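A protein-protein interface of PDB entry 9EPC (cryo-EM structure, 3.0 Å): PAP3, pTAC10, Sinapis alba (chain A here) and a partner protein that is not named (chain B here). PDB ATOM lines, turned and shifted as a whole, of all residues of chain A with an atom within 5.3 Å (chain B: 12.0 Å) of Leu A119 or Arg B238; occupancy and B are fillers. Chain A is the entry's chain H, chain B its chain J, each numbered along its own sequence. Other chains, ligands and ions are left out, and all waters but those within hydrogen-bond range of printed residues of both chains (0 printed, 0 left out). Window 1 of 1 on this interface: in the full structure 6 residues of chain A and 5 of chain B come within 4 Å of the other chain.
The backbone carbonyl oxygen (O) of Ser B233 lies within hydrogen-bond range of the guanidinium group (NE) of Arg B238 (3.1 Å).
The guanidinium group of Arg B238 sits close to the backbone carbonyl oxygen of Trp B234.
NE of Arg B238 lies within hydrogen-bond range of O of Ser B230 (3.5 Å).
The backbone NH (N) of Thr B229 lies within hydrogen-bond range of the side-chain carboxylate (OE1) of Glu B232.
Among the printed residues, merely in contact across the chains: Glu A91 with Trp B235 (3.4 Å), Phe A116 with Trp B234 (3.5 Å), Leu A119 with Trp B234 (3.9 Å), Arg A120 with Asp B231 (3.8 Å) and Pro A121 with Arg B238 (3.3 Å).
The backbone carbonyl oxygen (O) of Glu B232 lies close to the guanidinium group (NE) of Arg A120.
The guanidinium group (NH2) of Arg B238 lies within salt-bridge range of the side-chain carboxylate (OE2) of Glu A91, 3.6 Å away.
The backbone nitrogen (N) of Pro A121 sits close to the backbone carbonyl oxygen (O) of Asp B231, 3.4 Å away.
NH2 of Arg B238 is in hydrogen-bond range of O of Leu A119 (3.0 Å).
The guanidinium group (NE) of Arg A120 sits close to the indole nitrogen (NE1) of Trp B234 (3.0 Å).
Of chain B, only Trp B234 (3.9 Å) and Arg B238 (3.0 Å) come within 4 Å of Leu A119.
Of the printed residues of chain A, Arg B238 touches Glu A91 (3.6 Å), Leu A119 (3.0 Å) and Pro A121 (3.3 Å).
No residue of chain B comes within 4 Å of Pro A90.
Of chain B, only Trp B235 and Arg B238 come within 4 Å of Glu A91.
No residue of chain B comes within 4 Å of Phe A94.
Phe A116 touches just one residue of chain B: Trp B234 (3.5 Å).
No residue of chain B comes within 4 Å of Met A118.
Of chain B, only Asp B231 (3.2 Å) and Arg B238 (3.3 Å) come within 4 Å of Pro A121.
Printed residues of chain A within 4 Å of Asp B231: Arg A120 (3.8 Å) and Pro A121 (3.2 Å).
Of the printed residues of chain A, Trp B235 touches Glu A91 (3.4 Å).
The nearest residue of chain B that does not touch Leu A119 is Ser B233 (4.05 Å).
The nearest residue of chain A that does not touch Arg B238 is Arg A120 (4.7 Å).
Of the 18 printed residues of chain B, 5 touch a printed residue of chain A.
Hydrophobic or aromatic side chains of chain B within 4 Å of the printed part of chain A: Trp B234 and Trp B235.
Of the 10 printed residues of chain A, 5 touch a printed residue of chain B.
Hydrophobic or aromatic side chains of chain A that line the printed part of chain B: Phe A116, Leu A119 and Pro A121.
Among the printed residues, Asp or Glu carboxylates within 4 Å of a Lys or Arg side-chain nitrogen of the other chain: Glu A91 with Arg B238 (3.6 Å).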
ATOM      1  N   PRO A  90      -6.279  25.058  -8.908  1.00  0.00           N
ATOM      2  CA  PRO A  90      -7.061  26.204  -9.399  1.00  0.00           C
ATOM      3  C   PRO A  90      -8.520  25.875  -9.639  1.00  0.00           C
ATOM      4  O   PRO A  90      -9.381  26.742  -9.449  1.00  0.00           O
ATOM      5  CB  PRO A  90      -6.345  26.580 -10.701  1.00  0.00           C
ATOM      6  CG  PRO A  90      -4.953  26.127 -10.496  1.00  0.00           C
ATOM      7  CD  PRO A  90      -5.047  24.865  -9.691  1.00  0.00           C
ATOM      8  N   GLU A  91      -8.826  24.645 -10.055  1.00  0.00           N
ATOM      9  CA  GLU A  91     -10.218  24.251 -10.227  1.00  0.00           C
ATOM     10  C   GLU A  91     -10.923  24.115  -8.884  1.00  0.00           C
ATOM     11  O   GLU A  91     -12.084  24.514  -8.743  1.00  0.00           O
ATOM     12  CB  GLU A  91     -10.302  22.942 -11.010  1.00  0.00           C
ATOM     13  CG  GLU A  91      -9.796  23.026 -12.441  1.00  0.00           C
ATOM     14  CD  GLU A  91      -8.287  23.023 -12.534  1.00  0.00           C
ATOM     15  OE1 GLU A  91      -7.632  22.644 -11.543  1.00  0.00           O
ATOM     16  OE2 GLU A  91      -7.754  23.403 -13.597  1.00  0.00           O
ATOM     17  N   PHE A  94     -11.304  27.663  -7.310  1.00  0.00           N
ATOM     18  CA  PHE A  94     -12.397  28.388  -7.946  1.00  0.00           C
ATOM     19  C   PHE A  94     -13.750  27.928  -7.428  1.00  0.00           C
ATOM     20  O   PHE A  94     -14.679  28.735  -7.319  1.00  0.00           O
ATOM     21  CB  PHE A  94     -12.324  28.216  -9.461  1.00  0.00           C
ATOM     22  CG  PHE A  94     -13.540  28.706 -10.186  1.00  0.00           C
ATOM     23  CD1 PHE A  94     -13.738  30.056 -10.398  1.00  0.00           C
ATOM     24  CD2 PHE A  94     -14.482  27.815 -10.663  1.00  0.00           C
ATOM     25  CE1 PHE A  94     -14.853  30.509 -11.068  1.00  0.00           C
ATOM     26  CE2 PHE A  94     -15.599  28.262 -11.332  1.00  0.00           C
ATOM     27  CZ  PHE A  94     -15.784  29.611 -11.537  1.00  0.00           C
ATOM     28  N   ALA A 115      -9.889  33.935  -9.159  1.00  0.00           N
ATOM     29  CA  ALA A 115      -9.885  32.477  -9.207  1.00  0.00           C
ATOM     30  C   ALA A 115     -10.366  31.974 -10.559  1.00  0.00           C
ATOM     31  O   ALA A 115      -9.870  30.962 -11.067  1.00  0.00           O
ATOM     32  CB  ALA A 115     -10.752  31.909  -8.084  1.00  0.00           C
ATOM     33  N   PHE A 116     -11.338  32.666 -11.155  1.00  0.00           N
ATOM     34  CA  PHE A 116     -11.808  32.290 -12.483  1.00  0.00           C
ATOM     35  C   PHE A 116     -10.699  32.420 -13.516  1.00  0.00           C
ATOM     36  O   PHE A 116     -10.534  31.546 -14.374  1.00  0.00           O
ATOM     37  CB  PHE A 116     -13.009  33.150 -12.872  1.00  0.00           C
ATOM     38  CG  PHE A 116     -13.563  32.838 -14.229  1.00  0.00           C
ATOM     39  CD1 PHE A 116     -14.543  31.875 -14.384  1.00  0.00           C
ATOM     40  CD2 PHE A 116     -13.111  33.510 -15.350  1.00  0.00           C
ATOM     41  CE1 PHE A 116     -15.055  31.585 -15.628  1.00  0.00           C
ATOM     42  CE2 PHE A 116     -13.620  33.222 -16.595  1.00  0.00           C
ATOM     43  CZ  PHE A 116     -14.594  32.260 -16.733  1.00  0.00           C
ATOM     44  N   LYS A 117      -9.928  33.507 -13.453  1.00  0.00           N
ATOM     45  CA  LYS A 117      -8.866  33.711 -14.431  1.00  0.00           C
ATOM     46  C   LYS A 117      -7.732  32.712 -14.253  1.00  0.00           C
ATOM     47  O   LYS A 117      -7.016  32.413 -15.214  1.00  0.00           O
ATOM     48  CB  LYS A 117      -8.333  35.137 -14.338  1.00  0.00           C
ATOM     49  CG  LYS A 117      -9.346  36.200 -14.710  1.00  0.00           C
ATOM     50  CD  LYS A 117      -8.712  37.576 -14.717  1.00  0.00           C
ATOM     51  CE  LYS A 117      -9.693  38.630 -15.189  1.00  0.00           C
ATOM     52  NZ  LYS A 117      -9.072  39.982 -15.231  1.00  0.00           N
ATOM     53  N   MET A 118      -7.550  32.189 -13.042  1.00  0.00           N
ATOM     54  CA  MET A 118      -6.495  31.218 -12.790  1.00  0.00           C
ATOM     55  C   MET A 118      -6.832  29.827 -13.305  1.00  0.00           C
ATOM     56  O   MET A 118      -5.969  28.946 -13.262  1.00  0.00           O
ATOM     57  CB  MET A 118      -6.189  31.151 -11.293  1.00  0.00           C
ATOM     58  CG  MET A 118      -5.551  32.410 -10.738  1.00  0.00           C
ATOM     59  SD  MET A 118      -3.894  32.686 -11.388  1.00  0.00           S
ATOM     60  CE  MET A 118      -3.058  31.226 -10.783  1.00  0.00           C
ATOM     61  N   LEU A 119      -8.059  29.606 -13.782  1.00  0.00           N
ATOM     62  CA  LEU A 119      -8.411  28.314 -14.356  1.00  0.00           C
ATOM     63  C   LEU A 119      -7.593  27.999 -15.598  1.00  0.00           C
ATOM     64  O   LEU A 119      -7.441  26.823 -15.945  1.00  0.00           O
ATOM     65  CB  LEU A 119      -9.899  28.273 -14.692  1.00  0.00           C
ATOM     66  CG  LEU A 119     -10.840  28.345 -13.495  1.00  0.00           C
ATOM     67  CD1 LEU A 119     -12.273  28.421 -13.959  1.00  0.00           C
ATOM     68  CD2 LEU A 119     -10.635  27.145 -12.597  1.00  0.00           C
ATOM     69  N   ARG A 120      -7.068  29.017 -16.275  1.00  0.00           N
ATOM     70  CA  ARG A 120      -6.198  28.804 -17.418  1.00  0.00           C
ATOM     71  C   ARG A 120      -4.755  28.853 -16.951  1.00  0.00           C
ATOM     72  O   ARG A 120      -4.299  29.915 -16.501  1.00  0.00           O
ATOM     73  CB  ARG A 120      -6.446  29.862 -18.486  1.00  0.00           C
ATOM     74  CG  ARG A 120      -7.839  29.834 -19.065  1.00  0.00           C
ATOM     75  CD  ARG A 120      -8.074  31.014 -19.980  1.00  0.00           C
ATOM     76  NE  ARG A 120      -9.402  30.975 -20.575  1.00  0.00           N
ATOM     77  CZ  ARG A 120      -9.884  31.901 -21.390  1.00  0.00           C
ATOM     78  NH1 ARG A 120      -9.169  32.959 -21.731  1.00  0.00           N
ATOM     79  NH2 ARG A 120     -11.114  31.765 -21.875  1.00  0.00           N
ATOM     80  N   PRO A 121      -4.002  27.755 -17.031  1.00  0.00           N
ATOM     81  CA  PRO A 121      -2.589  27.811 -16.629  1.00  0.00           C
ATOM     82  C   PRO A 121      -1.765  28.777 -17.457  1.00  0.00           C
ATOM     83  O   PRO A 121      -0.708  29.216 -16.991  1.00  0.00           O
ATOM     84  CB  PRO A 121      -2.112  26.364 -16.809  1.00  0.00           C
ATOM     85  CG  PRO A 121      -3.104  25.737 -17.720  1.00  0.00           C
ATOM     86  CD  PRO A 121      -4.408  26.401 -17.429  1.00  0.00           C
ATOM     87  N   THR B 227      -5.659  26.803 -32.242  1.00  0.00           N
ATOM     88  CA  THR B 227      -6.657  26.985 -31.200  1.00  0.00           C
ATOM     89  C   THR B 227      -6.005  26.809 -29.831  1.00  0.00           C
ATOM     90  O   THR B 227      -4.779  26.734 -29.707  1.00  0.00           O
ATOM     91  CB  THR B 227      -7.819  26.012 -31.402  1.00  0.00           C
ATOM     92  OG1 THR B 227      -7.329  24.666 -31.361  1.00  0.00           O
ATOM     93  CG2 THR B 227      -8.485  26.259 -32.744  1.00  0.00           C
ATOM     94  N   LEU B 228      -6.842  26.760 -28.795  1.00  0.00           N
ATOM     95  CA  LEU B 228      -6.351  26.587 -27.436  1.00  0.00           C
ATOM     96  C   LEU B 228      -5.573  25.284 -27.312  1.00  0.00           C
ATOM     97  O   LEU B 228      -5.978  24.248 -27.842  1.00  0.00           O
ATOM     98  CB  LEU B 228      -7.521  26.605 -26.452  1.00  0.00           C
ATOM     99  CG  LEU B 228      -8.436  27.824 -26.563  1.00  0.00           C
ATOM    100  CD1 LEU B 228      -9.538  27.767 -25.522  1.00  0.00           C
ATOM    101  CD2 LEU B 228      -7.635  29.104 -26.428  1.00  0.00           C
ATOM    102  N   THR B 229      -4.446  25.346 -26.608  1.00  0.00           N
ATOM    103  CA  THR B 229      -3.509  24.234 -26.507  1.00  0.00           C
ATOM    104  C   THR B 229      -3.593  23.540 -25.151  1.00  0.00           C
ATOM    105  O   THR B 229      -2.577  23.136 -24.583  1.00  0.00           O
ATOM    106  CB  THR B 229      -2.082  24.707 -26.764  1.00  0.00           C
ATOM    107  OG1 THR B 229      -1.677  25.590 -25.713  1.00  0.00           O
ATOM    108  CG2 THR B 229      -2.002  25.442 -28.092  1.00  0.00           C
ATOM    109  N   SER B 230      -4.806  23.423 -24.608  1.00  0.00           N
ATOM    110  CA  SER B 230      -5.067  22.740 -23.343  1.00  0.00           C
ATOM    111  C   SER B 230      -4.371  23.422 -22.172  1.00  0.00           C
ATOM    112  O   SER B 230      -4.412  22.924 -21.044  1.00  0.00           O
ATOM    113  CB  SER B 230      -4.650  21.268 -23.419  1.00  0.00           C
ATOM    114  OG  SER B 230      -3.241  21.134 -23.404  1.00  0.00           O
ATOM    115  N   ASP B 231      -3.722  24.557 -22.431  1.00  0.00           N
ATOM    116  CA  ASP B 231      -3.187  25.410 -21.384  1.00  0.00           C
ATOM    117  C   ASP B 231      -3.766  26.811 -21.402  1.00  0.00           C
ATOM    118  O   ASP B 231      -3.733  27.485 -20.368  1.00  0.00           O
ATOM    119  CB  ASP B 231      -1.657  25.504 -21.482  1.00  0.00           C
ATOM    120  CG  ASP B 231      -0.965  24.311 -20.863  1.00  0.00           C
ATOM    121  OD1 ASP B 231      -1.668  23.427 -20.334  1.00  0.00           O
ATOM    122  OD2 ASP B 231       0.281  24.257 -20.903  1.00  0.00           O
ATOM    123  N   GLU B 232      -4.286  27.269 -22.534  1.00  0.00           N
ATOM    124  CA  GLU B 232      -5.077  28.486 -22.580  1.00  0.00           C
ATOM    125  C   GLU B 232      -6.552  28.213 -22.345  1.00  0.00           C
ATOM    126  O   GLU B 232      -7.365  29.136 -22.451  1.00  0.00           O
ATOM    127  CB  GLU B 232      -4.895  29.195 -23.925  1.00  0.00           C
ATOM    128  CG  GLU B 232      -3.454  29.475 -24.304  1.00  0.00           C
ATOM    129  CD  GLU B 232      -2.861  28.385 -25.168  1.00  0.00           C
ATOM    130  OE1 GLU B 232      -3.555  27.380 -25.421  1.00  0.00           O
ATOM    131  OE2 GLU B 232      -1.698  28.535 -25.598  1.00  0.00           O
ATOM    132  N   SER B 233      -6.913  26.971 -22.038  1.00  0.00           N
ATOM    133  CA  SER B 233      -8.298  26.560 -21.896  1.00  0.00           C
ATOM    134  C   SER B 233      -8.575  26.108 -20.472  1.00  0.00           C
ATOM    135  O   SER B 233      -7.694  25.578 -19.788  1.00  0.00           O
ATOM    136  CB  SER B 233      -8.636  25.425 -22.862  1.00  0.00           C
ATOM    137  OG  SER B 233      -9.945  24.940 -22.630  1.00  0.00           O
ATOM    138  N   TRP B 234      -9.812  26.317 -20.033  1.00  0.00           N
ATOM    139  CA  TRP B 234     -10.240  25.807 -18.745  1.00  0.00           C
ATOM    140  C   TRP B 234     -10.239  24.284 -18.763  1.00  0.00           C
ATOM    141  O   TRP B 234     -10.065  23.644 -19.801  1.00  0.00           O
ATOM    142  CB  TRP B 234     -11.646  26.296 -18.405  1.00  0.00           C
ATOM    143  CG  TRP B 234     -11.880  27.746 -18.638  1.00  0.00           C
ATOM    144  CD1 TRP B 234     -11.015  28.765 -18.392  1.00  0.00           C
ATOM    145  CD2 TRP B 234     -13.063  28.343 -19.172  1.00  0.00           C
ATOM    146  NE1 TRP B 234     -11.587  29.964 -18.735  1.00  0.00           N
ATOM    147  CE2 TRP B 234     -12.845  29.730 -19.220  1.00  0.00           C
ATOM    148  CE3 TRP B 234     -14.286  27.838 -19.617  1.00  0.00           C
ATOM    149  CZ2 TRP B 234     -13.804  30.618 -19.693  1.00  0.00           C
ATOM    150  CZ3 TRP B 234     -15.236  28.719 -20.085  1.00  0.00           C
ATOM    151  CH2 TRP B 234     -14.990  30.093 -20.120  1.00  0.00           C
ATOM    152  N   TRP B 235     -10.459  23.696 -17.592  1.00  0.00           N
ATOM    153  CA  TRP B 235     -10.821  22.292 -17.556  1.00  0.00           C
ATOM    154  C   TRP B 235     -12.183  22.123 -18.221  1.00  0.00           C
ATOM    155  O   TRP B 235     -12.838  23.093 -18.606  1.00  0.00           O
ATOM    156  CB  TRP B 235     -10.827  21.777 -16.121  1.00  0.00           C
ATOM    157  CG  TRP B 235     -12.033  22.178 -15.347  1.00  0.00           C
ATOM    158  CD1 TRP B 235     -12.261  23.380 -14.752  1.00  0.00           C
ATOM    159  CD2 TRP B 235     -13.182  21.371 -15.076  1.00  0.00           C
ATOM    160  NE1 TRP B 235     -13.482  23.373 -14.128  1.00  0.00           N
ATOM    161  CE2 TRP B 235     -14.067  22.149 -14.313  1.00  0.00           C
ATOM    162  CE3 TRP B 235     -13.546  20.063 -15.406  1.00  0.00           C
ATOM    163  CZ2 TRP B 235     -15.294  21.668 -13.875  1.00  0.00           C
ATOM    164  CZ3 TRP B 235     -14.764  19.588 -14.972  1.00  0.00           C
ATOM    165  CH2 TRP B 235     -15.624  20.386 -14.214  1.00  0.00           C
ATOM    166  N   ASN B 236     -12.604  20.872 -18.388  1.00  0.00           N
ATOM    167  CA  ASN B 236     -13.849  20.467 -19.038  1.00  0.00           C
ATOM    168  C   ASN B 236     -13.846  20.759 -20.533  1.00  0.00           C
ATOM    169  O   ASN B 236     -14.787  20.360 -21.227  1.00  0.00           O
ATOM    170  CB  ASN B 236     -15.095  21.104 -18.396  1.00  0.00           C
ATOM    171  CG  ASN B 236     -15.551  22.368 -19.106  1.00  0.00           C
ATOM    172  OD1 ASN B 236     -16.415  22.326 -19.979  1.00  0.00           O
ATOM    173  ND2 ASN B 236     -14.979  23.500 -18.723  1.00  0.00           N
ATOM    174  N   TRP B 237     -12.816  21.422 -21.057  1.00  0.00           N
ATOM    175  CA  TRP B 237     -12.640  21.567 -22.490  1.00  0.00           C
ATOM    176  C   TRP B 237     -11.295  21.045 -22.969  1.00  0.00           C
ATOM    177  O   TRP B 237     -11.067  20.992 -24.181  1.00  0.00           O
ATOM    178  CB  TRP B 237     -12.795  23.033 -22.918  1.00  0.00           C
ATOM    179  CG  TRP B 237     -14.191  23.552 -22.805  1.00  0.00           C
ATOM    180  CD1 TRP B 237     -14.604  24.632 -22.089  1.00  0.00           C
ATOM    181  CD2 TRP B 237     -15.363  23.011 -23.425  1.00  0.00           C
ATOM    182  NE1 TRP B 237     -15.958  24.802 -22.226  1.00  0.00           N
ATOM    183  CE2 TRP B 237     -16.447  23.818 -23.041  1.00  0.00           C
ATOM    184  CE3 TRP B 237     -15.598  21.923 -24.269  1.00  0.00           C
ATOM    185  CZ2 TRP B 237     -17.746  23.572 -23.470  1.00  0.00           C
ATOM    186  CZ3 TRP B 237     -16.887  21.681 -24.693  1.00  0.00           C
ATOM    187  CH2 TRP B 237     -17.945  22.501 -24.294  1.00  0.00           C
ATOM    188  N   ARG B 238     -10.402  20.670 -22.060  1.00  0.00           N
ATOM    189  CA  ARG B 238      -9.131  20.080 -22.440  1.00  0.00           C
ATOM    190  C   ARG B 238      -9.325  18.642 -22.896  1.00  0.00           C
ATOM    191  O   ARG B 238     -10.222  17.935 -22.431  1.00  0.00           O
ATOM    192  CB  ARG B 238      -8.152  20.114 -21.269  1.00  0.00           C
ATOM    193  CG  ARG B 238      -7.871  21.495 -20.732  1.00  0.00           C
ATOM    194  CD  ARG B 238      -7.142  21.413 -19.411  1.00  0.00           C
ATOM    195  NE  ARG B 238      -7.049  22.712 -18.759  1.00  0.00           N
ATOM    196  CZ  ARG B 238      -6.739  22.883 -17.483  1.00  0.00           C
ATOM    197  NH1 ARG B 238      -6.488  21.855 -16.690  1.00  0.00           N
ATOM    198  NH2 ARG B 238      -6.687  24.115 -16.988  1.00  0.00           N
ATOM    199  N   LYS B 239      -8.474  18.213 -23.819  1.00  0.00           N
ATOM    200  CA  LYS B 239      -8.461  16.812 -24.196  1.00  0.00           C
ATOM    201  C   LYS B 239      -8.015  15.973 -23.002  1.00  0.00           C
ATOM    202  O   LYS B 239      -7.146  16.401 -22.234  1.00  0.00           O
ATOM    203  CB  LYS B 239      -7.533  16.580 -25.388  1.00  0.00           C
ATOM    204  CG  LYS B 239      -8.028  17.203 -26.677  1.00  0.00           C
ATOM    205  CD  LYS B 239      -9.424  16.709 -27.013  1.00  0.00           C
ATOM    206  CE  LYS B 239      -9.945  17.343 -28.289  1.00  0.00           C
ATOM    207  NZ  LYS B 239     -11.310  16.856 -28.626  1.00  0.00           N
ATOM    208  N   PRO B 240      -8.584  14.780 -22.813  1.00  0.00           N
ATOM    209  CA  PRO B 240      -8.333  14.021 -21.580  1.00  0.00           C
ATOM    210  C   PRO B 240      -6.899  13.548 -21.405  1.00  0.00           C
ATOM    211  O   PRO B 240      -6.627  12.842 -20.426  1.00  0.00           O
ATOM    212  CB  PRO B 240      -9.286  12.824 -21.710  1.00  0.00           C
ATOM    213  CG  PRO B 240     -10.321  13.259 -22.688  1.00  0.00           C
ATOM    214  CD  PRO B 240      -9.605  14.140 -23.656  1.00  0.00           C
ATOM    215  N   GLU B 241      -5.984  13.878 -22.318  1.00  0.00           N
ATOM    216  CA  GLU B 241      -4.577  13.482 -22.291  1.00  0.00           C
ATOM    217  C   GLU B 241      -4.416  11.982 -22.497  1.00  0.00           C
ATOM    218  O   GLU B 241      -3.286  11.497 -22.616  1.00  0.00           O
ATOM    219  CB  GLU B 241      -3.879  13.913 -20.990  1.00  0.00           C
ATOM    220  CG  GLU B 241      -2.356  13.920 -21.030  1.00  0.00           C
ATOM    221  CD  GLU B 241      -1.752  12.680 -20.396  1.00  0.00           C
ATOM    222  OE1 GLU B 241      -2.513  11.879 -19.814  1.00  0.00           O
ATOM    223  OE2 GLU B 241      -0.518  12.504 -20.483  1.00  0.00           O
ATOM    224  N   LYS B 242      -5.512  11.235 -22.583  1.00  0.00           N
ATOM    225  CA  LYS B 242      -5.473   9.791 -22.772  1.00  0.00           C
ATOM    226  C   LYS B 242      -6.822   9.387 -23.335  1.00  0.00           C
ATOM    227  O   LYS B 242      -7.844   9.567 -22.666  1.00  0.00           O
ATOM    228  CB  LYS B 242      -5.191   9.076 -21.455  1.00  0.00           C
ATOM    229  CG  LYS B 242      -5.052   7.574 -21.570  1.00  0.00           C
ATOM    230  CD  LYS B 242      -4.942   6.934 -20.196  1.00  0.00           C
ATOM    231  CE  LYS B 242      -3.773   7.501 -19.409  1.00  0.00           C
ATOM    232  NZ  LYS B 242      -2.471   7.238 -20.075  1.00  0.00           N
ATOM    233  N   GLU B 243      -6.831   8.864 -24.559  1.00  0.00           N
ATOM    234  CA  GLU B 243      -8.086   8.580 -25.241  1.00  0.00           C
ATOM    235  C   GLU B 243      -8.944   7.637 -24.411  1.00  0.00           C
ATOM    236  O   GLU B 243      -8.456   6.656 -23.851  1.00  0.00           O
ATOM    237  CB  GLU B 243      -7.811   7.976 -26.617  1.00  0.00           C
ATOM    238  CG  GLU B 243      -9.040   7.859 -27.493  1.00  0.00           C
ATOM    239  CD  GLU B 243      -8.698   7.601 -28.943  1.00  0.00           C
ATOM    240  OE1 GLU B 243      -7.608   7.054 -29.210  1.00  0.00           O
ATOM    241  OE2 GLU B 243      -9.514   7.955 -29.818  1.00  0.00           O
ATOM    242  N   GLN B 244     -10.232   7.949 -24.322  1.00  0.00           N
ATOM    243  CA  GLN B 244     -11.150   7.226 -23.458  1.00  0.00           C
ATOM    244  C   GLN B 244     -11.965   6.225 -24.262  1.00  0.00           C
ATOM    245  O   GLN B 244     -12.426   6.526 -25.366  1.00  0.00           O
ATOM    246  CB  GLN B 244     -12.084   8.196 -22.735  1.00  0.00           C
ATOM    247  CG  GLN B 244     -11.364   9.249 -21.918  1.00  0.00           C
ATOM    248  CD  GLN B 244     -10.578   8.657 -20.769  1.00  0.00           C
ATOM    249  OE1 GLN B 244     -10.959   7.636 -20.202  1.00  0.00           O
ATOM    250  NE2 GLN B 244      -9.469   9.296 -20.421  1.00  0.00           N
